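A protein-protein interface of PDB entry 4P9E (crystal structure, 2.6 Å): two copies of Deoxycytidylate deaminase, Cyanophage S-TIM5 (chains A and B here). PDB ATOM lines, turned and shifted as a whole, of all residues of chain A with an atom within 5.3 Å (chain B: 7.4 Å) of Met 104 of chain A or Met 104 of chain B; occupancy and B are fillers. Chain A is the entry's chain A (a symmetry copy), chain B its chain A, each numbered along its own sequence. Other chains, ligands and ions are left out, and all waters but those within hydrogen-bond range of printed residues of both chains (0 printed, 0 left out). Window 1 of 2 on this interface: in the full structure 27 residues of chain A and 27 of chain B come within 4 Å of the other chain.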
ATOM      1  N   LEU A  69      35.476   5.544  25.185  1.00  0.00           N
ATOM      2  CA  LEU A  69      34.027   5.465  25.103  1.00  0.00           C
ATOM      3  C   LEU A  69      33.485   6.564  24.203  1.00  0.00           C
ATOM      4  O   LEU A  69      34.005   7.675  24.190  1.00  0.00           O
ATOM      5  CB  LEU A  69      33.423   5.635  26.499  1.00  0.00           C
ATOM      6  CG  LEU A  69      34.048   4.728  27.545  1.00  0.00           C
ATOM      7  CD1 LEU A  69      34.565   5.548  28.721  1.00  0.00           C
ATOM      8  CD2 LEU A  69      33.047   3.705  27.984  1.00  0.00           C
ATOM      9  N   GLN A  73      27.866   6.259  24.826  1.00  0.00           N
ATOM     10  CA  GLN A  73      28.256   5.335  25.886  1.00  0.00           C
ATOM     11  C   GLN A  73      28.430   5.992  27.276  1.00  0.00           C
ATOM     12  O   GLN A  73      27.971   5.455  28.285  1.00  0.00           O
ATOM     13  CB  GLN A  73      29.506   4.570  25.478  1.00  0.00           C
ATOM     14  CG  GLN A  73      29.195   3.491  24.473  1.00  0.00           C
ATOM     15  CD  GLN A  73      30.409   3.005  23.696  1.00  0.00           C
ATOM     16  OE1 GLN A  73      31.542   3.399  23.964  1.00  0.00           O
ATOM     17  NE2 GLN A  73      30.165   2.150  22.703  1.00  0.00           N
ATOM     18  N   LEU A  76      24.847   7.098  28.539  1.00  0.00           N
ATOM     19  CA  LEU A  76      24.228   5.848  28.946  1.00  0.00           C
ATOM     20  C   LEU A  76      24.743   5.301  30.277  1.00  0.00           C
ATOM     21  O   LEU A  76      23.967   4.895  31.136  1.00  0.00           O
ATOM     22  CB  LEU A  76      24.460   4.805  27.861  1.00  0.00           C
ATOM     23  CG  LEU A  76      23.804   3.445  28.120  1.00  0.00           C
ATOM     24  CD1 LEU A  76      22.300   3.583  28.213  1.00  0.00           C
ATOM     25  CD2 LEU A  76      24.177   2.491  27.022  1.00  0.00           C
ATOM     26  N   VAL A  77      26.058   5.260  30.447  1.00  0.00           N
ATOM     27  CA  VAL A  77      26.613   4.801  31.715  1.00  0.00           C
ATOM     28  C   VAL A  77      26.203   5.717  32.879  1.00  0.00           C
ATOM     29  O   VAL A  77      25.899   5.246  33.969  1.00  0.00           O
ATOM     30  CB  VAL A  77      28.155   4.587  31.630  1.00  0.00           C
ATOM     31  CG1 VAL A  77      28.815   4.700  32.995  1.00  0.00           C
ATOM     32  CG2 VAL A  77      28.463   3.236  30.984  1.00  0.00           C
ATOM     33  N   ASP A 100      27.180   0.417  17.266  1.00  0.00           N
ATOM     34  CA  ASP A 100      27.253  -0.093  18.640  1.00  0.00           C
ATOM     35  C   ASP A 100      26.468   0.780  19.627  1.00  0.00           C
ATOM     36  O   ASP A 100      25.870   0.285  20.586  1.00  0.00           O
ATOM     37  CB  ASP A 100      28.708  -0.215  19.115  1.00  0.00           C
ATOM     38  CG  ASP A 100      29.578  -1.053  18.172  1.00  0.00           C
ATOM     39  OD1 ASP A 100      29.043  -2.014  17.551  1.00  0.00           O
ATOM     40  OD2 ASP A 100      30.797  -0.742  18.052  1.00  0.00           O
ATOM     41  N   CYS A 101      26.486   2.084  19.395  1.00  0.00           N
ATOM     42  CA  CYS A 101      25.700   2.969  20.218  1.00  0.00           C
ATOM     43  C   CYS A 101      24.227   2.833  19.848  1.00  0.00           C
ATOM     44  O   CYS A 101      23.361   2.785  20.713  1.00  0.00           O
ATOM     45  CB  CYS A 101      26.206   4.405  20.094  1.00  0.00           C
ATOM     46  SG  CYS A 101      27.879   4.634  20.784  1.00  0.00           S
ATOM     47  N   SER A 102      23.945   2.720  18.560  1.00  0.00           N
ATOM     48  CA  SER A 102      22.576   2.527  18.097  1.00  0.00           C
ATOM     49  C   SER A 102      21.816   1.346  18.722  1.00  0.00           C
ATOM     50  O   SER A 102      20.670   1.509  19.121  1.00  0.00           O
ATOM     51  CB  SER A 102      22.556   2.427  16.578  1.00  0.00           C
ATOM     52  OG  SER A 102      22.949   3.662  16.014  1.00  0.00           O
ATOM     53  N   LYS A 103      22.449   0.175  18.809  1.00  0.00           N
ATOM     54  CA  LYS A 103      21.852  -1.001  19.444  1.00  0.00           C
ATOM     55  C   LYS A 103      21.380  -0.679  20.845  1.00  0.00           C
ATOM     56  O   LYS A 103      20.333  -1.156  21.296  1.00  0.00           O
ATOM     57  CB  LYS A 103      22.884  -2.113  19.636  1.00  0.00           C
ATOM     58  CG  LYS A 103      23.570  -2.657  18.424  1.00  0.00           C
ATOM     59  CD  LYS A 103      24.570  -3.766  18.825  1.00  0.00           C
ATOM     60  CE  LYS A 103      25.605  -3.301  19.835  1.00  0.00           C
ATOM     61  NZ  LYS A 103      26.818  -4.163  19.814  1.00  0.00           N
ATOM     62  N   MET A 104      22.205   0.089  21.549  1.00  0.00           N
ATOM     63  CA  MET A 104      22.016   0.304  22.972  1.00  0.00           C
ATOM     64  C   MET A 104      20.969   1.366  23.220  1.00  0.00           C
ATOM     65  O   MET A 104      20.111   1.229  24.101  1.00  0.00           O
ATOM     66  CB  MET A 104      23.336   0.680  23.628  1.00  0.00           C
ATOM     67  CG  MET A 104      24.359  -0.444  23.586  1.00  0.00           C
ATOM     68  SD  MET A 104      25.651  -0.253  24.829  1.00  0.00           S
ATOM     69  CE  MET A 104      26.787   0.822  23.974  1.00  0.00           C
ATOM     70  N   ILE A 105      21.056   2.419  22.420  1.00  0.00           N
ATOM     71  CA  ILE A 105      20.066   3.472  22.397  1.00  0.00           C
ATOM     72  C   ILE A 105      18.663   2.890  22.169  1.00  0.00           C
ATOM     73  O   ILE A 105      17.715   3.255  22.867  1.00  0.00           O
ATOM     74  CB  ILE A 105      20.435   4.494  21.314  1.00  0.00           C
ATOM     75  CG1 ILE A 105      21.764   5.151  21.662  1.00  0.00           C
ATOM     76  CG2 ILE A 105      19.369   5.546  21.145  1.00  0.00           C
ATOM     77  CD1 ILE A 105      22.419   5.851  20.502  1.00  0.00           C
ATOM     78  N   ALA A 106      18.528   1.971  21.216  1.00  0.00           N
ATOM     79  CA  ALA A 106      17.210   1.403  20.914  1.00  0.00           C
ATOM     80  C   ALA A 106      16.701   0.522  22.046  1.00  0.00           C
ATOM     81  O   ALA A 106      15.530   0.586  22.440  1.00  0.00           O
ATOM     82  CB  ALA A 106      17.246   0.620  19.633  1.00  0.00           C
ATOM     83  N   GLN A 107      17.592  -0.313  22.558  1.00  0.00           N
ATOM     84  CA  GLN A 107      17.260  -1.197  23.650  1.00  0.00           C
ATOM     85  C   GLN A 107      16.973  -0.414  24.943  1.00  0.00           C
ATOM     86  O   GLN A 107      16.268  -0.894  25.832  1.00  0.00           O
ATOM     87  CB  GLN A 107      18.390  -2.199  23.855  1.00  0.00           C
ATOM     88  CG  GLN A 107      17.993  -3.431  24.634  1.00  0.00           C
ATOM     89  CD  GLN A 107      17.118  -4.388  23.844  1.00  0.00           C
ATOM     90  OE1 GLN A 107      15.967  -4.088  23.539  1.00  0.00           O
ATOM     91  NE2 GLN A 107      17.660  -5.556  23.520  1.00  0.00           N
ATOM     92  N   ALA A 108      17.501   0.805  25.031  1.00  0.00           N
ATOM     93  CA  ALA A 108      17.330   1.639  26.219  1.00  0.00           C
ATOM     94  C   ALA A 108      15.976   2.338  26.268  1.00  0.00           C
ATOM     95  O   ALA A 108      15.615   2.944  27.271  1.00  0.00           O
ATOM     96  CB  ALA A 108      18.452   2.657  26.307  1.00  0.00           C
ATOM     97  N   GLY A 109      15.231   2.250  25.177  1.00  0.00           N
ATOM     98  CA  GLY A 109      13.944   2.904  25.078  1.00  0.00           C
ATOM     99  C   GLY A 109      14.065   4.385  24.790  1.00  0.00           C
ATOM    100  O   GLY A 109      13.160   5.162  25.104  1.00  0.00           O
ATOM    101  N   PRO B  49      18.337  -6.914  19.492  1.00  0.00           N
ATOM    102  CA  PRO B  49      17.485  -5.986  20.229  1.00  0.00           C
ATOM    103  C   PRO B  49      16.027  -6.344  20.062  1.00  0.00           C
ATOM    104  O   PRO B  49      15.653  -6.928  19.054  1.00  0.00           O
ATOM    105  CB  PRO B  49      17.777  -4.652  19.553  1.00  0.00           C
ATOM    106  CG  PRO B  49      19.164  -4.781  19.090  1.00  0.00           C
ATOM    107  CD  PRO B  49      19.336  -6.207  18.677  1.00  0.00           C
ATOM    108  N   PHE B  67      24.743  -6.080  15.163  1.00  0.00           N
ATOM    109  CA  PHE B  67      23.634  -5.540  15.946  1.00  0.00           C
ATOM    110  C   PHE B  67      23.160  -6.388  17.131  1.00  0.00           C
ATOM    111  O   PHE B  67      22.167  -6.062  17.776  1.00  0.00           O
ATOM    112  CB  PHE B  67      22.486  -5.083  15.041  1.00  0.00           C
ATOM    113  CG  PHE B  67      22.815  -3.825  14.287  1.00  0.00           C
ATOM    114  CD1 PHE B  67      22.709  -2.582  14.905  1.00  0.00           C
ATOM    115  CD2 PHE B  67      23.298  -3.882  12.985  1.00  0.00           C
ATOM    116  CE1 PHE B  67      23.046  -1.418  14.225  1.00  0.00           C
ATOM    117  CE2 PHE B  67      23.633  -2.717  12.298  1.00  0.00           C
ATOM    118  CZ  PHE B  67      23.505  -1.485  12.921  1.00  0.00           C
ATOM    119  N   LEU B  69      23.615  -7.450  20.955  1.00  0.00           N
ATOM    120  CA  LEU B  69      24.176  -6.937  22.195  1.00  0.00           C
ATOM    121  C   LEU B  69      24.781  -8.066  23.012  1.00  0.00           C
ATOM    122  O   LEU B  69      24.257  -9.175  23.031  1.00  0.00           O
ATOM    123  CB  LEU B  69      23.073  -6.273  23.023  1.00  0.00           C
ATOM    124  CG  LEU B  69      22.248  -5.268  22.237  1.00  0.00           C
ATOM    125  CD1 LEU B  69      20.766  -5.616  22.318  1.00  0.00           C
ATOM    126  CD2 LEU B  69      22.518  -3.887  22.751  1.00  0.00           C
ATOM    127  N   HIS B  70      25.884  -7.778  23.690  1.00  0.00           N
ATOM    128  CA  HIS B  70      26.459  -8.722  24.622  1.00  0.00           C
ATOM    129  C   HIS B  70      25.593  -8.736  25.868  1.00  0.00           C
ATOM    130  O   HIS B  70      24.850  -7.792  26.121  1.00  0.00           O
ATOM    131  CB  HIS B  70      27.883  -8.321  24.960  1.00  0.00           C
ATOM    132  CG  HIS B  70      28.804  -8.351  23.784  1.00  0.00           C
ATOM    133  ND1 HIS B  70      30.102  -7.896  23.847  1.00  0.00           N
ATOM    134  CD2 HIS B  70      28.620  -8.791  22.521  1.00  0.00           C
ATOM    135  CE1 HIS B  70      30.673  -8.041  22.663  1.00  0.00           C
ATOM    136  NE2 HIS B  70      29.797  -8.583  21.845  1.00  0.00           N
ATOM    137  N   GLU B  72      26.387  -8.294  28.841  1.00  0.00           N
ATOM    138  CA  GLU B  72      26.757  -7.214  29.737  1.00  0.00           C
ATOM    139  C   GLU B  72      26.119  -5.912  29.270  1.00  0.00           C
ATOM    140  O   GLU B  72      25.631  -5.134  30.079  1.00  0.00           O
ATOM    141  CB  GLU B  72      28.289  -7.068  29.830  1.00  0.00           C
ATOM    142  CG  GLU B  72      29.069  -8.331  30.232  1.00  0.00           C
ATOM    143  CD  GLU B  72      29.453  -9.214  29.040  1.00  0.00           C
ATOM    144  OE1 GLU B  72      28.634  -9.379  28.100  1.00  0.00           O
ATOM    145  OE2 GLU B  72      30.581  -9.758  29.053  1.00  0.00           O
ATOM    146  N   GLN B  73      26.123  -5.670  27.963  1.00  0.00           N
ATOM    147  CA  GLN B  73      25.365  -4.566  27.382  1.00  0.00           C
ATOM    148  C   GLN B  73      23.857  -4.572  27.730  1.00  0.00           C
ATOM    149  O   GLN B  73      23.286  -3.533  28.061  1.00  0.00           O
ATOM    150  CB  GLN B  73      25.584  -4.519  25.877  1.00  0.00           C
ATOM    151  CG  GLN B  73      26.933  -3.949  25.528  1.00  0.00           C
ATOM    152  CD  GLN B  73      27.398  -4.283  24.118  1.00  0.00           C
ATOM    153  OE1 GLN B  73      26.667  -4.874  23.326  1.00  0.00           O
ATOM    154  NE2 GLN B  73      28.641  -3.916  23.810  1.00  0.00           N
ATOM    155  N   ASN B  74      23.232  -5.742  27.676  1.00  0.00           N
ATOM    156  CA  ASN B  74      21.838  -5.872  28.092  1.00  0.00           C
ATOM    157  C   ASN B  74      21.577  -5.555  29.569  1.00  0.00           C
ATOM    158  O   ASN B  74      20.656  -4.796  29.904  1.00  0.00           O
ATOM    159  CB  ASN B  74      21.298  -7.249  27.738  1.00  0.00           C
ATOM    160  CG  ASN B  74      20.669  -7.278  26.373  1.00  0.00           C
ATOM    161  OD1 ASN B  74      20.016  -6.316  25.964  1.00  0.00           O
ATOM    162  ND2 ASN B  74      20.858  -8.375  25.653  1.00  0.00           N
ATOM    163  N   LEU B  76      23.510  -3.758  31.586  1.00  0.00           N
ATOM    164  CA  LEU B  76      23.763  -2.329  31.657  1.00  0.00           C
ATOM    165  C   LEU B  76      22.599  -1.464  31.170  1.00  0.00           C
ATOM    166  O   LEU B  76      22.220  -0.494  31.817  1.00  0.00           O
ATOM    167  CB  LEU B  76      24.999  -2.003  30.829  1.00  0.00           C
ATOM    168  CG  LEU B  76      25.431  -0.534  30.862  1.00  0.00           C
ATOM    169  CD1 LEU B  76      25.782  -0.108  32.271  1.00  0.00           C
ATOM    170  CD2 LEU B  76      26.604  -0.336  29.945  1.00  0.00           C
ATOM    171  N   VAL B  77      22.043  -1.793  30.012  1.00  0.00           N
ATOM    172  CA  VAL B  77      20.893  -1.044  29.518  1.00  0.00           C
ATOM    173  C   VAL B  77      19.687  -1.170  30.462  1.00  0.00           C
ATOM    174  O   VAL B  77      18.974  -0.201  30.697  1.00  0.00           O
ATOM    175  CB  VAL B  77      20.549  -1.415  28.044  1.00  0.00           C
ATOM    176  CG1 VAL B  77      19.089  -1.138  27.721  1.00  0.00           C
ATOM    177  CG2 VAL B  77      21.473  -0.667  27.084  1.00  0.00           C
ATOM    178  N   ILE B  86      23.931   1.458  39.273  1.00  0.00           N
ATOM    179  CA  ILE B  86      24.794   0.324  38.990  1.00  0.00           C
ATOM    180  C   ILE B  86      26.114   0.446  39.772  1.00  0.00           C
ATOM    181  O   ILE B  86      26.843  -0.532  39.951  1.00  0.00           O
ATOM    182  CB  ILE B  86      25.046   0.170  37.471  1.00  0.00           C
ATOM    183  CG1 ILE B  86      25.598  -1.224  37.160  1.00  0.00           C
ATOM    184  CG2 ILE B  86      25.961   1.256  36.947  1.00  0.00           C
ATOM    185  CD1 ILE B  86      25.891  -1.457  35.715  1.00  0.00           C
ATOM    186  N   CYS B  98      34.462  -8.694  26.858  1.00  0.00           N
ATOM    187  CA  CYS B  98      35.229  -8.108  25.763  1.00  0.00           C
ATOM    188  C   CYS B  98      35.740  -6.732  26.165  1.00  0.00           C
ATOM    189  O   CYS B  98      35.335  -6.208  27.196  1.00  0.00           O
ATOM    190  CB  CYS B  98      34.357  -8.029  24.496  1.00  0.00           C
ATOM    191  SG  CYS B  98      33.143  -6.678  24.437  1.00  0.00           S
ATOM    192  N   PRO B  99      36.651  -6.143  25.370  1.00  0.00           N
ATOM    193  CA  PRO B  99      37.108  -4.794  25.710  1.00  0.00           C
ATOM    194  C   PRO B  99      36.001  -3.729  25.730  1.00  0.00           C
ATOM    195  O   PRO B  99      36.090  -2.830  26.561  1.00  0.00           O
ATOM    196  CB  PRO B  99      38.129  -4.490  24.606  1.00  0.00           C
ATOM    197  CG  PRO B  99      38.660  -5.810  24.241  1.00  0.00           C
ATOM    198  CD  PRO B  99      37.477  -6.728  24.295  1.00  0.00           C
ATOM    199  N   ASP B 100      34.995  -3.830  24.858  1.00  0.00           N
ATOM    200  CA  ASP B 100      33.922  -2.831  24.786  1.00  0.00           C
ATOM    201  C   ASP B 100      33.006  -2.873  26.015  1.00  0.00           C
ATOM    202  O   ASP B 100      32.510  -1.843  26.481  1.00  0.00           O
ATOM    203  CB  ASP B 100      33.077  -3.008  23.517  1.00  0.00           C
ATOM    204  CG  ASP B 100      33.916  -3.005  22.233  1.00  0.00           C
ATOM    205  OD1 ASP B 100      34.957  -2.291  22.193  1.00  0.00           O
ATOM    206  OD2 ASP B 100      33.529  -3.723  21.268  1.00  0.00           O
ATOM    207  N   CYS B 101      32.772  -4.072  26.529  1.00  0.00           N
ATOM    208  CA  CYS B 101      31.998  -4.194  27.738  1.00  0.00           C
ATOM    209  C   CYS B 101      32.841  -3.750  28.929  1.00  0.00           C
ATOM    210  O   CYS B 101      32.365  -3.046  29.812  1.00  0.00           O
ATOM    211  CB  CYS B 101      31.468  -5.618  27.893  1.00  0.00           C
ATOM    212  SG  CYS B 101      30.245  -6.068  26.616  1.00  0.00           S
ATOM    213  N   SER B 102      34.111  -4.120  28.929  1.00  0.00           N
ATOM    214  CA  SER B 102      35.023  -3.703  29.988  1.00  0.00           C
ATOM    215  C   SER B 102      35.104  -2.190  30.247  1.00  0.00           C
ATOM    216  O   SER B 102      35.061  -1.772  31.397  1.00  0.00           O
ATOM    217  CB  SER B 102      36.410  -4.272  29.726  1.00  0.00           C
ATOM    218  OG  SER B 102      36.374  -5.682  29.824  1.00  0.00           O
ATOM    219  N   LYS B 103      35.214  -1.383  29.191  1.00  0.00           N
ATOM    220  CA  LYS B 103      35.233   0.075  29.310  1.00  0.00           C
ATOM    221  C   LYS B 103      34.033   0.571  30.088  1.00  0.00           C
ATOM    222  O   LYS B 103      34.125   1.514  30.880  1.00  0.00           O
ATOM    223  CB  LYS B 103      35.104   0.746  27.942  1.00  0.00           C
ATOM    224  CG  LYS B 103      36.141   0.448  26.909  1.00  0.00           C
ATOM    225  CD  LYS B 103      35.836   1.218  25.603  1.00  0.00           C
ATOM    226  CE  LYS B 103      34.455   0.921  25.043  1.00  0.00           C
ATOM    227  NZ  LYS B 103      34.374   1.230  23.590  1.00  0.00           N
ATOM    228  N   MET B 104      32.890  -0.042  29.799  1.00  0.00           N
ATOM    229  CA  MET B 104      31.615   0.459  30.282  1.00  0.00           C
ATOM    230  C   MET B 104      31.376   0.025  31.711  1.00  0.00           C
ATOM    231  O   MET B 104      30.912   0.808  32.550  1.00  0.00           O
ATOM    232  CB  MET B 104      30.487  -0.011  29.375  1.00  0.00           C
ATOM    233  CG  MET B 104      30.573   0.571  27.974  1.00  0.00           C
ATOM    234  SD  MET B 104      28.994   0.521  27.105  1.00  0.00           S
ATOM    235  CE  MET B 104      29.032  -1.129  26.430  1.00  0.00           C
ATOM    236  N   ILE B 105      31.707  -1.232  31.965  1.00  0.00           N
ATOM    237  CA  ILE B 105      31.693  -1.794  33.296  1.00  0.00           C
ATOM    238  C   ILE B 105      32.537  -0.938  34.253  1.00  0.00           C
ATOM    239  O   ILE B 105      32.098  -0.625  35.362  1.00  0.00           O
ATOM    240  CB  ILE B 105      32.196  -3.243  33.243  1.00  0.00           C
ATOM    241  CG1 ILE B 105      31.244  -4.085  32.404  1.00  0.00           C
ATOM    242  CG2 ILE B 105      32.336  -3.841  34.620  1.00  0.00           C
ATOM    243  CD1 ILE B 105      31.832  -5.392  31.945  1.00  0.00           C
ATOM    244  N   ALA B 106      33.731  -0.538  33.825  1.00  0.00           N
ATOM    245  CA  ALA B 106      34.608   0.247  34.702  1.00  0.00           C
ATOM    246  C   ALA B 106      34.059   1.644  34.949  1.00  0.00           C
ATOM    247  O   ALA B 106      34.062   2.151  36.077  1.00  0.00           O
ATOM    248  CB  ALA B 106      35.994   0.335  34.130  1.00  0.00           C
ATOM    249  N   GLN B 107      33.599   2.269  33.876  1.00  0.00           N
ATOM    250  CA  GLN B 107      33.030   3.594  33.957  1.00  0.00           C
ATOM    251  C   GLN B 107      31.714   3.593  34.753  1.00  0.00           C
ATOM    252  O   GLN B 107      31.310   4.617  35.310  1.00  0.00           O
ATOM    253  CB  GLN B 107      32.822   4.145  32.551  1.00  0.00           C
ATOM    254  CG  GLN B 107      32.667   5.647  32.491  1.00  0.00           C
ATOM    255  CD  GLN B 107      33.966   6.396  32.729  1.00  0.00           C
ATOM    256  OE1 GLN B 107      34.503   6.395  33.833  1.00  0.00           O
ATOM    257  NE2 GLN B 107      34.469   7.054  31.692  1.00  0.00           N
ATOM    258  N   ALA B 108      31.061   2.435  34.828  1.00  0.00           N
ATOM    259  CA  ALA B 108      29.784   2.310  35.527  1.00  0.00           C
ATOM    260  C   ALA B 108      29.939   2.197  37.039  1.00  0.00           C
ATOM    261  O   ALA B 108      28.963   2.243  37.778  1.00  0.00           O
ATOM    262  CB  ALA B 108      29.009   1.121  34.986  1.00  0.00           C
ATOM    263  N   GLY B 109      31.175   2.044  37.491  1.00  0.00           N
ATOM    264  CA  GLY B 109      31.455   1.882  38.902  1.00  0.00           C
ATOM    265  C   GLY B 109      31.179   0.477  39.392  1.00  0.00           C
ATOM    266  O   GLY B 109      30.930   0.265  40.581  1.00  0.00           O
ATOM    267  N   VAL B 110      31.185  -0.483  38.475  1.00  0.00           N
ATOM    268  CA  VAL B 110      31.068  -1.880  38.858  1.00  0.00           C
ATOM    269  C   VAL B 110      32.284  -2.227  39.710  1.00  0.00           C
ATOM    270  O   VAL B 110      33.416  -1.995  39.319  1.00  0.00           O
ATOM    271  CB  VAL B 110      30.936  -2.787  37.636  1.00  0.00           C
ATOM    272  CG1 VAL B 110      31.129  -4.242  37.997  1.00  0.00           C
ATOM    273  CG2 VAL B 110      29.572  -2.585  37.001  1.00  0.00           C
ATOM    274  N   LEU B 128      40.099  -4.051  32.979  1.00  0.00           N
ATOM    275  CA  LEU B 128      39.264  -3.952  34.164  1.00  0.00           C
ATOM    276  C   LEU B 128      40.149  -3.772  35.402  1.00  0.00           C
ATOM    277  O   LEU B 128      39.817  -3.015  36.320  1.00  0.00           O
ATOM    278  CB  LEU B 128      38.386  -5.198  34.314  1.00  0.00           C
ATOM    279  CG  LEU B 128      37.185  -5.428  33.388  1.00  0.00           C
ATOM    280  CD1 LEU B 128      36.842  -6.895  33.327  1.00  0.00           C
ATOM    281  CD2 LEU B 128      35.958  -4.662  33.840  1.00  0.00           C
ATOM    282  N   LEU B 131      41.874  -0.439  35.600  1.00  0.00           N
ATOM    283  CA  LEU B 131      40.882   0.577  35.954  1.00  0.00           C
ATOM    284  C   LEU B 131      40.273   0.422  37.346  1.00  0.00           C
ATOM    285  O   LEU B 131      39.386   1.187  37.718  1.00  0.00           O
ATOM    286  CB  LEU B 131      39.780   0.633  34.892  1.00  0.00           C
ATOM    287  CG  LEU B 131      40.256   1.152  33.536  1.00  0.00           C
ATOM    288  CD1 LEU B 131      39.156   1.097  32.492  1.00  0.00           C
ATOM    289  CD2 LEU B 131      40.788   2.564  33.682  1.00  0.00           C
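OD1 of Asn 74 of chain B is in hydrogen-bond range of NE2 of Gln 107 of chain A, 3.5 Å away.
The backbone NH of His 70 of chain B is in hydrogen-bond range of the side-chain amide oxygen of Gln 73 of chain B, 3.0 Å away. The side-chain amino group (NZ) of Lys 103 of chain B lies within salt-bridge range of the side-chain carboxylate (OD1) of Asp 100 of chain B (3.8 Å). The side-chain carboxylate (OD1) of Asp 100 of chain A is in salt-bridge range of the side-chain amino group (NZ) of Lys 103 of chain A (3.8 Å).
Leu 69 of chain A touches Lys 103 of chain B (CD2 to CB, 3.6 Å). Leu 69 of chain A touches Gln 107 of chain B (CD1 to NE2, 3.3 Å). NZ of Lys 103 of chain B touches OE1 of Gln 73 of chain A, 3.6 Å away. O of Gln 107 of chain B touches CG1 of Val 77 of chain A, 3.4 Å away. CG1 of Val 77 of chain A touches CA of Ala 108 of chain B, at 3.6 Å. Lys 103 of chain A touches Leu 69 of chain B. Lys 103 of chain A touches Gln 73 of chain B (NZ to OE1, 3.6 Å). Met 104 of chain A touches Gln 73 of chain B. Gln 107 of chain A touches Pro 49 of chain B (NE2 to CA, 3.3 Å). Gln 107 of chain A touches Val 77 of chain B.
Of the printed residues of chain B, Met 104 of chain A touches Leu 69 (3.99 Å), Gln 73 (3.97 Å), Val 77 (3.8 Å) and Met 104 (3.8 Å). Printed residues of chain A within 4 Å of Met 104 of chain B: Leu 69 (3.99 Å), Gln 73 (3.97 Å), Val 77 (3.8 Å) and Met 104 (3.8 Å). Printed residues of chain A within 4 Å of Ala 108 of chain B: Val 77. Printed residues of chain B within 4 Å of Gln 73 of chain A: Lys 103 and Met 104. Of the printed residues of chain A, Asn 74 of chain B touches Gln 107. Printed residues of chain B within 4 Å of Gln 107 of chain A: Pro 49 (3.3 Å), Leu 69 (3.3 Å), Asn 74 (3.5 Å) and Val 77 (3.4 Å). Of the printed residues of chain A, Lys 103 of chain B touches Leu 69 and Gln 73. Gly 109 of chain A touches none of the printed residues of chain B. The nearest printed residue of chain B that does not touch Met 104 of chain A is Leu 76 of chain B (5.2 Å). The nearest printed residue of chain A that does not touch Met 104 of chain B is Leu 76 of chain A (5.2 Å).
Of the 14 printed residues of chain A, 7 touch a printed residue of chain B. Printed residues of chain A that touch a printed residue of chain B: Leu 69, Gln 73, Val 77, Lys 103, Met 104, Gln 107 and Ala 108. Of the 25 printed residues of chain B, 10 touch a printed residue of chain A. Hydrophobic or aromatic side chains of chain B that line the printed part of chain A: Phe 67, Leu 69, Val 77 and Met 104. Among the printed residues, 20 pairs touch across the chains.
Leu 69 of chain A touches Lys 103 of chain B, and with the chains exchanged Lys 103 of chain A touches Leu 69 of chain B. Leu 69 of chain A touches Gln 107 of chain B, and with the chains exchanged Gln 107 of chain A touches Leu 69 of chain B. Val 77 of chain A touches Gln 107 of chain B, and with the chains exchanged Gln 107 of chain A touches Val 77 of chain B. Val 77 of chain A touches Ala 108 of chain B, and with the chains exchanged Ala 108 of chain A touches Val 77 of chain B. 14 positions are printed for both chains.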
